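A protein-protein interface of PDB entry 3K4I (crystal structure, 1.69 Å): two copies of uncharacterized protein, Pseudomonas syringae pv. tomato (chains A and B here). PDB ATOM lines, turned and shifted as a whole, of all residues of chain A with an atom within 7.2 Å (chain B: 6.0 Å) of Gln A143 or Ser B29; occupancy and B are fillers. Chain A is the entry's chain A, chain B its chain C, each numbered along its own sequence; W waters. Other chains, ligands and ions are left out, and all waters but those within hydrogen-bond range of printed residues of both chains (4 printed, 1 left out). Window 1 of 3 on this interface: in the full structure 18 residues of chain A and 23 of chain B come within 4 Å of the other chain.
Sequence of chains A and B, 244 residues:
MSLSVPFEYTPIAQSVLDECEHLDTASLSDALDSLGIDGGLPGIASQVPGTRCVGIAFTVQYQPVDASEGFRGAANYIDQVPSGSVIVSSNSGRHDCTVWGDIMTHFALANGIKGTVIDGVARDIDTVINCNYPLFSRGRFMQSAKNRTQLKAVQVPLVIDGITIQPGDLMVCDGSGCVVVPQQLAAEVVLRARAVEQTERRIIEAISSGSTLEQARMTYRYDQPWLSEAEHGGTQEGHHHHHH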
ATOM      1  N   HIS A  95      19.159  -1.525  18.002  1.00  0.00           N
ATOM      2  CA  HIS A  95      18.911  -2.040  16.668  1.00  0.00           C
ATOM      3  C   HIS A  95      19.558  -3.418  16.475  1.00  0.00           C
ATOM      4  O   HIS A  95      19.478  -3.972  15.389  1.00  0.00           O
ATOM      5  CB  HIS A  95      19.443  -1.043  15.637  1.00  0.00           C
ATOM      6  CG  HIS A  95      18.448   0.000  15.246  1.00  0.00           C
ATOM      7  ND1 HIS A  95      18.360   1.226  15.880  1.00  0.00           N
ATOM      8  CD2 HIS A  95      17.499   0.008  14.281  1.00  0.00           C
ATOM      9  CE1 HIS A  95      17.398   1.942  15.319  1.00  0.00           C
ATOM     10  NE2 HIS A  95      16.867   1.234  14.342  1.00  0.00           N
ATOM     11  N   ASP A  96      20.188  -3.953  17.516  1.00  0.00           N
ATOM     12  CA  ASP A  96      20.978  -5.191  17.420  1.00  0.00           C
ATOM     13  C   ASP A  96      20.233  -6.442  17.916  1.00  0.00           C
ATOM     14  O   ASP A  96      20.731  -7.556  17.798  1.00  0.00           O
ATOM     15  CB  ASP A  96      22.351  -5.038  18.124  1.00  0.00           C
ATOM     16  CG  ASP A  96      22.227  -4.803  19.629  1.00  0.00           C
ATOM     17  OD1 ASP A  96      21.235  -4.167  20.057  1.00  0.00           O
ATOM     18  OD2 ASP A  96      23.128  -5.251  20.370  1.00  0.00           O
ATOM     19  N   CYS A  97      19.040  -6.239  18.462  1.00  0.00           N
ATOM     20  CA  CYS A  97      18.229  -7.343  19.008  1.00  0.00           C
ATOM     21  C   CYS A  97      16.780  -6.888  19.020  1.00  0.00           C
ATOM     22  O   CYS A  97      16.503  -5.683  18.955  1.00  0.00           O
ATOM     23  CB  CYS A  97      18.671  -7.746  20.419  1.00  0.00           C
ATOM     24  SG  CYS A  97      18.706  -6.348  21.640  1.00  0.00           S
ATOM     25  N   THR A  98      15.865  -7.853  19.054  1.00  0.00           N
ATOM     26  CA  THR A  98      14.429  -7.583  18.900  1.00  0.00           C
ATOM     27  C   THR A  98      13.696  -8.019  20.181  1.00  0.00           C
ATOM     28  O   THR A  98      14.135  -8.956  20.859  1.00  0.00           O
ATOM     29  CB  THR A  98      13.853  -8.391  17.718  1.00  0.00           C
ATOM     30  OG1 THR A  98      14.211  -9.760  17.903  1.00  0.00           O
ATOM     31  CG2 THR A  98      14.410  -7.847  16.384  1.00  0.00           C
ATOM     32  N   VAL A  99      12.599  -7.331  20.500  1.00  0.00           N
ATOM     33  CA  VAL A  99      11.789  -7.628  21.705  1.00  0.00           C
ATOM     34  C   VAL A  99      10.318  -7.945  21.346  1.00  0.00           C
ATOM     35  O   VAL A  99       9.415  -7.832  22.173  1.00  0.00           O
ATOM     36  CB  VAL A  99      11.918  -6.526  22.824  1.00  0.00           C
ATOM     37  CG1 VAL A  99      13.345  -6.485  23.368  1.00  0.00           C
ATOM     38  CG2 VAL A  99      11.549  -5.152  22.299  1.00  0.00           C
ATOM     39  N   VAL A 121      13.441  -2.512  18.140  1.00  0.00           N
ATOM     40  CA  VAL A 121      13.037  -3.172  16.879  1.00  0.00           C
ATOM     41  C   VAL A 121      12.363  -4.503  17.127  1.00  0.00           C
ATOM     42  O   VAL A 121      12.444  -5.048  18.207  1.00  0.00           O
ATOM     43  CB  VAL A 121      14.206  -3.292  15.870  1.00  0.00           C
ATOM     44  CG1 VAL A 121      14.666  -1.871  15.394  1.00  0.00           C
ATOM     45  CG2 VAL A 121      15.378  -4.039  16.444  1.00  0.00           C
ATOM     46  N   ALA A 122      11.685  -5.010  16.093  1.00  0.00           N
ATOM     47  CA  ALA A 122      10.917  -6.250  16.147  1.00  0.00           C
ATOM     48  C   ALA A 122      11.365  -7.190  15.035  1.00  0.00           C
ATOM     49  O   ALA A 122      11.886  -6.750  14.024  1.00  0.00           O
ATOM     50  CB  ALA A 122       9.398  -5.959  15.960  1.00  0.00           C
ATOM     51  N   ARG A 123      11.099  -8.482  15.220  1.00  0.00           N
ATOM     52  CA  ARG A 123      11.359  -9.478  14.179  1.00  0.00           C
ATOM     53  C   ARG A 123      10.090 -10.147  13.700  1.00  0.00           C
ATOM     54  O   ARG A 123       9.024  -9.808  14.153  1.00  0.00           O
ATOM     55  CB  ARG A 123      12.363 -10.526  14.647  1.00  0.00           C
ATOM     56  CG  ARG A 123      11.920 -11.484  15.755  1.00  0.00           C
ATOM     57  CD  ARG A 123      13.127 -12.386  15.987  1.00  0.00           C
ATOM     58  NE  ARG A 123      12.929 -13.486  16.927  1.00  0.00           N
ATOM     59  CZ  ARG A 123      13.863 -14.400  17.195  1.00  0.00           C
ATOM     60  NH1 ARG A 123      15.078 -14.348  16.620  1.00  0.00           N
ATOM     61  NH2 ARG A 123      13.570 -15.383  18.059  1.00  0.00           N
ATOM     62  N   PHE A 141      14.372  -6.147  12.482  1.00  0.00           N
ATOM     63  CA  PHE A 141      15.629  -6.904  12.511  1.00  0.00           C
ATOM     64  C   PHE A 141      15.290  -8.347  12.850  1.00  0.00           C
ATOM     65  O   PHE A 141      14.121  -8.673  12.941  1.00  0.00           O
ATOM     66  CB  PHE A 141      16.629  -6.285  13.504  1.00  0.00           C
ATOM     67  CG  PHE A 141      18.077  -6.750  13.309  1.00  0.00           C
ATOM     68  CD1 PHE A 141      18.869  -7.059  14.412  1.00  0.00           C
ATOM     69  CD2 PHE A 141      18.662  -6.785  12.042  1.00  0.00           C
ATOM     70  CE1 PHE A 141      20.229  -7.432  14.242  1.00  0.00           C
ATOM     71  CE2 PHE A 141      20.038  -7.210  11.850  1.00  0.00           C
ATOM     72  CZ  PHE A 141      20.802  -7.536  12.966  1.00  0.00           C
ATOM     73  N   MET A 142      16.292  -9.226  12.986  1.00  0.00           N
ATOM     74  CA  MET A 142      15.957 -10.643  13.246  1.00  0.00           C
ATOM     75  C   MET A 142      16.666 -11.269  14.420  1.00  0.00           C
ATOM     76  O   MET A 142      16.304 -12.372  14.839  1.00  0.00           O
ATOM     77  CB  MET A 142      16.105 -11.529  11.958  1.00  0.00           C
ATOM     78  CG  MET A 142      17.530 -12.066  11.616  1.00  0.00           C
ATOM     79  SD  MET A 142      18.828 -10.597  11.509  1.00  0.00           S
ATOM     80  CE  MET A 142      18.161  -9.798   9.862  1.00  0.00           C
ATOM     81  N   GLN A 143      17.667 -10.593  14.980  1.00  0.00           N
ATOM     82  CA  GLN A 143      18.433 -11.195  16.078  1.00  0.00           C
ATOM     83  C   GLN A 143      17.643 -11.224  17.368  1.00  0.00           C
ATOM     84  O   GLN A 143      16.967 -10.244  17.744  1.00  0.00           O
ATOM     85  CB  GLN A 143      19.783 -10.460  16.243  1.00  0.00           C
ATOM     86  CG  GLN A 143      20.782 -10.872  15.141  1.00  0.00           C
ATOM     87  CD  GLN A 143      22.150 -10.230  15.222  1.00  0.00           C
ATOM     88  OE1 GLN A 143      23.002 -10.498  14.396  1.00  0.00           O
ATOM     89  NE2 GLN A 143      22.375  -9.381  16.234  1.00  0.00           N
ATOM     90  N   SER A 144      17.658 -12.388  18.008  1.00  0.00           N
ATOM     91  CA  SER A 144      16.935 -12.595  19.270  1.00  0.00           C
ATOM     92  C   SER A 144      17.414 -11.729  20.434  1.00  0.00           C
ATOM     93  O   SER A 144      18.582 -11.376  20.498  1.00  0.00           O
ATOM     94  CB  SER A 144      17.097 -14.042  19.713  1.00  0.00           C
ATOM     95  OG  SER A 144      16.362 -14.287  20.898  1.00  0.00           O
ATOM     96  N   ALA A 145      16.511 -11.479  21.382  1.00  0.00           N
ATOM     97  CA  ALA A 145      16.881 -10.857  22.671  1.00  0.00           C
ATOM     98  C   ALA A 145      17.826 -11.725  23.501  1.00  0.00           C
ATOM     99  O   ALA A 145      18.582 -11.215  24.344  1.00  0.00           O
ATOM    100  CB  ALA A 145      15.621 -10.533  23.500  1.00  0.00           C
ATOM    101  N   LYS A 146      17.756 -13.041  23.295  1.00  0.00           N
ATOM    102  CA  LYS A 146      18.543 -13.974  24.098  1.00  0.00           C
ATOM    103  C   LYS A 146      20.024 -13.601  24.127  1.00  0.00           C
ATOM    104  O   LYS A 146      20.683 -13.423  23.086  1.00  0.00           O
ATOM    105  CB  LYS A 146      18.345 -15.423  23.607  1.00  0.00           C
ATOM    106  CG  LYS A 146      19.115 -16.474  24.411  1.00  0.00           C
ATOM    107  CD  LYS A 146      19.054 -17.858  23.748  1.00  0.00           C
ATOM    108  CE  LYS A 146      19.717 -18.953  24.602  1.00  0.00           C
ATOM    109  NZ  LYS A 146      19.089 -19.090  25.961  1.00  0.00           N
ATOM    110  N   ARG A 148      21.373 -10.929  24.759  1.00  0.00           N
ATOM    111  CA  ARG A 148      21.642  -9.547  24.283  1.00  0.00           C
ATOM    112  C   ARG A 148      20.930  -8.512  25.139  1.00  0.00           C
ATOM    113  O   ARG A 148      21.521  -7.484  25.509  1.00  0.00           O
ATOM    114  CB  ARG A 148      21.199  -9.334  22.827  1.00  0.00           C
ATOM    115  CG  ARG A 148      21.887 -10.254  21.813  1.00  0.00           C
ATOM    116  CD  ARG A 148      21.577  -9.820  20.390  1.00  0.00           C
ATOM    117  NE  ARG A 148      22.437 -10.524  19.451  1.00  0.00           N
ATOM    118  CZ  ARG A 148      22.200 -11.732  18.928  1.00  0.00           C
ATOM    119  NH1 ARG A 148      21.084 -12.422  19.206  1.00  0.00           N
ATOM    120  NH2 ARG A 148      23.104 -12.252  18.111  1.00  0.00           N
ATOM    121  N   ASP B  24      12.662 -18.761   8.066  1.00  0.00           N
ATOM    122  CA  ASP B  24      12.671 -17.318   8.291  1.00  0.00           C
ATOM    123  C   ASP B  24      14.065 -16.894   8.740  1.00  0.00           C
ATOM    124  O   ASP B  24      14.815 -17.702   9.325  1.00  0.00           O
ATOM    125  CB  ASP B  24      11.730 -16.991   9.461  1.00  0.00           C
ATOM    126  CG  ASP B  24      10.264 -17.263   9.158  1.00  0.00           C
ATOM    127  OD1 ASP B  24       9.492 -17.413  10.122  1.00  0.00           O
ATOM    128  OD2 ASP B  24       9.865 -17.302   7.976  1.00  0.00           O
ATOM    129  N   THR B  25      14.404 -15.628   8.496  1.00  0.00           N
ATOM    130  CA  THR B  25      15.659 -15.079   9.031  1.00  0.00           C
ATOM    131  C   THR B  25      15.808 -15.281  10.530  1.00  0.00           C
ATOM    132  O   THR B  25      16.933 -15.489  11.006  1.00  0.00           O
ATOM    133  CB  THR B  25      15.827 -13.598   8.668  1.00  0.00           C
ATOM    134  OG1 THR B  25      14.628 -12.894   8.990  1.00  0.00           O
ATOM    135  CG2 THR B  25      16.123 -13.461   7.151  1.00  0.00           C
ATOM    136  N   ALA B  26      14.707 -15.201  11.284  1.00  0.00           N
ATOM    137  CA  ALA B  26      14.777 -15.424  12.735  1.00  0.00           C
ATOM    138  C   ALA B  26      15.276 -16.825  13.103  1.00  0.00           C
ATOM    139  O   ALA B  26      16.109 -16.969  14.001  1.00  0.00           O
ATOM    140  CB  ALA B  26      13.437 -15.109  13.418  1.00  0.00           C
ATOM    141  N   SER B  27      14.765 -17.867  12.431  1.00  0.00           N
ATOM    142  CA  SER B  27      15.196 -19.220  12.738  1.00  0.00           C
ATOM    143  C   SER B  27      16.695 -19.391  12.457  1.00  0.00           C
ATOM    144  O   SER B  27      17.420 -19.987  13.257  1.00  0.00           O
ATOM    145  CB  SER B  27      14.399 -20.242  11.924  1.00  0.00           C
ATOM    146  OG  SER B  27      13.021 -19.882  11.949  1.00  0.00           O
ATOM    147  N   LEU B  28      17.135 -18.851  11.317  1.00  0.00           N
ATOM    148  CA  LEU B  28      18.516 -18.979  10.903  1.00  0.00           C
ATOM    149  C   LEU B  28      19.431 -18.226  11.843  1.00  0.00           C
ATOM    150  O   LEU B  28      20.483 -18.730  12.213  1.00  0.00           O
ATOM    151  CB  LEU B  28      18.702 -18.490   9.465  1.00  0.00           C
ATOM    152  CG  LEU B  28      18.112 -19.536   8.497  1.00  0.00           C
ATOM    153  CD1 LEU B  28      17.831 -18.901   7.170  1.00  0.00           C
ATOM    154  CD2 LEU B  28      19.064 -20.743   8.362  1.00  0.00           C
ATOM    155  N   SER B  29      18.976 -17.048  12.269  1.00  0.00           N
ATOM    156  CA  SER B  29      19.734 -16.251  13.239  1.00  0.00           C
ATOM    157  C   SER B  29      19.844 -16.952  14.608  1.00  0.00           C
ATOM    158  O   SER B  29      20.934 -17.011  15.200  1.00  0.00           O
ATOM    159  CB  SER B  29      19.094 -14.881  13.388  1.00  0.00           C
ATOM    160  OG  SER B  29      19.841 -14.086  14.318  1.00  0.00           O
ATOM    161  N   ASP B  30      18.748 -17.526  15.090  1.00  0.00           N
ATOM    162  CA  ASP B  30      18.777 -18.287  16.370  1.00  0.00           C
ATOM    163  C   ASP B  30      19.721 -19.497  16.261  1.00  0.00           C
ATOM    164  O   ASP B  30      20.467 -19.806  17.194  1.00  0.00           O
ATOM    165  CB  ASP B  30      17.355 -18.733  16.768  1.00  0.00           C
ATOM    166  CG  ASP B  30      16.449 -17.563  17.145  1.00  0.00           C
ATOM    167  OD1 ASP B  30      16.909 -16.397  17.158  1.00  0.00           O
ATOM    168  OD2 ASP B  30      15.231 -17.804  17.388  1.00  0.00           O
ATOM    169  N   ALA B  31      19.748 -20.134  15.091  1.00  0.00           N
ATOM    170  CA  ALA B  31      20.651 -21.265  14.850  1.00  0.00           C
ATOM    171  C   ALA B  31      22.116 -20.819  14.878  1.00  0.00           C
ATOM    172  O   ALA B  31      22.972 -21.458  15.495  1.00  0.00           O
ATOM    173  CB  ALA B  31      20.325 -21.926  13.509  1.00  0.00           C
ATOM    174  N   LEU B  32      22.396 -19.736  14.177  1.00  0.00           N
ATOM    175  CA  LEU B  32      23.735 -19.156  14.217  1.00  0.00           C
ATOM    176  C   LEU B  32      24.138 -18.813  15.648  1.00  0.00           C
ATOM    177  O   LEU B  32      25.249 -19.124  16.055  1.00  0.00           O
ATOM    178  CB  LEU B  32      23.821 -17.932  13.346  1.00  0.00           C
ATOM    179  CG  LEU B  32      23.921 -18.251  11.858  1.00  0.00           C
ATOM    180  CD1 LEU B  32      23.595 -16.939  11.106  1.00  0.00           C
ATOM    181  CD2 LEU B  32      25.322 -18.748  11.476  1.00  0.00           C
ATOM    182  N   ASP B  33      23.218 -18.206  16.400  1.00  0.00           N
ATOM    183  CA  ASP B  33      23.524 -17.784  17.769  1.00  0.00           C
ATOM    184  C   ASP B  33      23.931 -18.992  18.605  1.00  0.00           C
ATOM    185  O   ASP B  33      24.797 -18.892  19.470  1.00  0.00           O
ATOM    186  CB  ASP B  33      22.298 -17.141  18.436  1.00  0.00           C
ATOM    187  CG  ASP B  33      22.059 -15.718  18.000  1.00  0.00           C
ATOM    188  OD1 ASP B  33      22.868 -15.167  17.217  1.00  0.00           O
ATOM    189  OD2 ASP B  33      21.035 -15.159  18.458  1.00  0.00           O
ATOM    190  N   SER B  34      23.285 -20.140  18.358  1.00  0.00           N
ATOM    191  CA  SER B  34      23.615 -21.384  19.066  1.00  0.00           C
ATOM    192  C   SER B  34      24.995 -21.908  18.724  1.00  0.00           C
ATOM    193  O   SER B  34      25.523 -22.796  19.410  1.00  0.00           O
ATOM    194  CB  SER B  34      22.538 -22.479  18.837  1.00  0.00           C
ATOM    195  OG  SER B  34      22.630 -23.039  17.550  1.00  0.00           O
ATOM    196  N   ILE B  37      27.687 -17.188  16.734  1.00  0.00           N
ATOM    197  CA  ILE B  37      27.966 -16.337  15.570  1.00  0.00           C
ATOM    198  C   ILE B  37      26.782 -15.404  15.316  1.00  0.00           C
ATOM    199  O   ILE B  37      25.630 -15.839  15.327  1.00  0.00           O
ATOM    200  CB  ILE B  37      28.200 -17.238  14.322  1.00  0.00           C
ATOM    201  CG1 ILE B  37      29.537 -17.976  14.460  1.00  0.00           C
ATOM    202  CG2 ILE B  37      28.154 -16.447  12.986  1.00  0.00           C
ATOM    203  CD1 ILE B  37      29.595 -19.190  13.563  1.00  0.00           C
ATOM    204  N   ASP B  38      27.065 -14.118  15.154  1.00  0.00           N
ATOM    205  CA  ASP B  38      26.064 -13.136  14.741  1.00  0.00           C
ATOM    206  C   ASP B  38      25.961 -13.179  13.254  1.00  0.00           C
ATOM    207  O   ASP B  38      26.994 -13.222  12.584  1.00  0.00           O
ATOM    208  CB  ASP B  38      26.572 -11.714  15.078  1.00  0.00           C
ATOM    209  CG  ASP B  38      26.476 -11.372  16.551  1.00  0.00           C
ATOM    210  OD1 ASP B  38      25.817 -12.101  17.299  1.00  0.00           O
ATOM    211  OD2 ASP B  38      27.057 -10.329  16.968  1.00  0.00           O
ATOM    212  N   GLY B  39      24.741 -13.140  12.723  1.00  0.00           N
ATOM    213  CA  GLY B  39      24.589 -13.164  11.269  1.00  0.00           C
ATOM    214  C   GLY B  39      23.828 -11.996  10.683  1.00  0.00           C
ATOM    215  O   GLY B  39      23.835 -11.810   9.487  1.00  0.00           O
ATOM    216  N   GLY B  40      23.162 -11.205  11.516  1.00  0.00           N
ATOM    217  CA  GLY B  40      22.306 -10.124  10.981  1.00  0.00           C
ATOM    218  C   GLY B  40      23.049  -8.899  10.510  1.00  0.00           C
ATOM    219  O   GLY B  40      24.068  -8.524  11.099  1.00  0.00           O
ATOM    220  N   LEU B  41      22.552  -8.302   9.430  1.00  0.00           N
ATOM    221  CA  LEU B  41      23.118  -7.063   8.889  1.00  0.00           C
ATOM    222  C   LEU B  41      22.216  -5.889   9.296  1.00  0.00           C
ATOM    223  O   LEU B  41      21.238  -5.559   8.608  1.00  0.00           O
ATOM    224  CB  LEU B  41      23.254  -7.169   7.355  1.00  0.00           C
ATOM    225  CG  LEU B  41      24.191  -8.284   6.826  1.00  0.00           C
ATOM    226  CD1 LEU B  41      24.253  -8.240   5.326  1.00  0.00           C
ATOM    227  CD2 LEU B  41      25.603  -8.078   7.357  1.00  0.00           C
ATOM    228  N   ILE B 163      30.431  -7.815  10.382  1.00  0.00           N
ATOM    229  CA  ILE B 163      30.053  -9.148   9.895  1.00  0.00           C
ATOM    230  C   ILE B 163      30.762  -9.396   8.584  1.00  0.00           C
ATOM    231  O   ILE B 163      30.615  -8.647   7.643  1.00  0.00           O
ATOM    232  CB  ILE B 163      28.517  -9.258   9.684  1.00  0.00           C
ATOM    233  CG1 ILE B 163      27.773  -8.827  10.954  1.00  0.00           C
ATOM    234  CG2 ILE B 163      28.081 -10.686   9.265  1.00  0.00           C
ATOM    235  CD1 ILE B 163      28.094  -9.708  12.138  1.00  0.00           C
ATOM    236  N   VAL B 179      20.425 -12.087   6.734  1.00  0.00           N
ATOM    237  CA  VAL B 179      21.301 -12.925   7.583  1.00  0.00           C
ATOM    238  C   VAL B 179      22.391 -13.579   6.725  1.00  0.00           C
ATOM    239  O   VAL B 179      22.111 -14.062   5.604  1.00  0.00           O
ATOM    240  CB  VAL B 179      20.504 -14.037   8.302  1.00  0.00           C
ATOM    241  CG1 VAL B 179      21.406 -14.932   9.129  1.00  0.00           C
ATOM    242  CG2 VAL B 179      19.421 -13.455   9.185  1.00  0.00           C
ATOM    243  N   VAL B 189      23.602 -25.110  10.205  1.00  0.00           N
ATOM    244  CA  VAL B 189      22.714 -24.005  10.588  1.00  0.00           C
ATOM    245  C   VAL B 189      21.279 -24.255  10.096  1.00  0.00           C
ATOM    246  O   VAL B 189      20.310 -24.023  10.815  1.00  0.00           O
ATOM    247  CB  VAL B 189      23.270 -22.655  10.100  1.00  0.00           C
ATOM    248  CG1 VAL B 189      22.228 -21.564  10.233  1.00  0.00           C
ATOM    249  CG2 VAL B 189      24.547 -22.340  10.889  1.00  0.00           C
HETATM  250  O   HOH W   1      20.740 -15.240  21.170  1.00  0.00           O
HETATM  251  O   HOH W   2      18.960 -14.588  16.828  1.00  0.00           O
HETATM  252  O   HOH W   3      24.677  -8.542  13.624  1.00  0.00           O
HETATM  253  O   HOH W   4      24.821  -8.992  18.451  1.00  0.00           O
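The guanidinium group of Arg A123 lies within salt-bridge range of the side-chain carboxylate of Asp B30 (2.8 Å).
The guanidinium group (NH1) of Arg A148 is in salt-bridge range of the side-chain carboxylate (OD2) of Asp B33, at 2.8 Å.
The side-chain amide oxygen of Gln A143 is in hydrogen-bond range of the backbone NH of Gly B40.
The guanidinium group (NH2) of Arg A148 lies within salt-bridge range of the side-chain carboxylate (OD1) of Asp B38, 2.8 Å away.
O of Asp A96 sits at hydrogen-bond distance from NE2 of Gln A143 (2.9 Å).
The guanidinium group (NH1) of Arg A123 lies within hydrogen-bond range of the backbone carbonyl oxygen (O) of Met A142, at 2.9 Å.
The side-chain hydroxyl (OG) of Ser A144 sits at hydrogen-bond distance from the backbone NH (N) of Lys A146 (3.0 Å).
The backbone carbonyl oxygen (O) of Ser A144 sits at hydrogen-bond distance from the guanidinium group (NH1) of Arg A148, at 3.0 Å.
NE2 of Gln A143 sits close to NE of Arg A148 (3.4 Å).
OG1 of Thr A98 is in hydrogen-bond range of O of Gln A143 (2.8 Å).
Among the printed residues, pairs that only touch across the chains: Met A142 with Val B179 (3.4 Å), Gln A143 with Ser B29 (3.4 Å), Ser A144 with Asp B30 (3.5 Å), Met A142 with Thr B25 (3.5 Å), Met A142 with Gly B40 (3.5 Å), Gln A143 with Gly B39 (3.6 Å), Phe A141 with Gly B40 (3.6 Å), Phe A141 with Leu B41 (3.6 Å), Met A142 with Ser B29 (3.7 Å), Arg A123 with Ala B26 (3.7 Å), Gln A143 with Asp B38 (3.8 Å) and Met A142 with Ala B26 (3.99 Å).
Gln A143 touches four residues of chain B.
Printed residues of chain A within 4 Å of Asp B30: Arg A123 (2.8 Å) and Ser A144 (3.5 Å).
Of the printed residues of chain B, Arg A148 touches Asp B33 and Asp B38.
Of the printed residues of chain A, Val B179 touches Met A142.
Leu B32 touches none of the printed residues of chain A.
The nearest residue of chain A that does not touch Ser B29 is Ser A144 (4.6 Å).
The nearest printed residue of chain A that does not touch Asp B33 is Ser A144 (4.3 Å).
Hydrophobic or aromatic side chains of chain B within 4 Å of the printed part of chain A: Ala B26 and Val B179.
No position is printed for both chains.
Water W3 lies within hydrogen-bond range of the backbone carbonyl oxygen of Gly B40 (2.6 Å) and the side-chain amide oxygen of Gln A143 (2.7 Å).
Water W1 lies within hydrogen-bond range of O of Lys A146 (2.6 Å), OD2 of Asp B33 (2.7 Å) and NH1 of Arg A148 (3.5 Å).
Water W2 lies within hydrogen-bond range of OD2 of Asp B33 (2.7 Å), OG of Ser B29 (2.7 Å), OD1 of Asp B30 (2.8 Å) and N of Ser A144 (2.8 Å).
Water W4 lies within hydrogen-bond range of the side-chain carboxylate (OD2) of Asp B38, the guanidinium group (NE) of Arg A148 and the side-chain amide nitrogen (NE2) of Gln A143.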
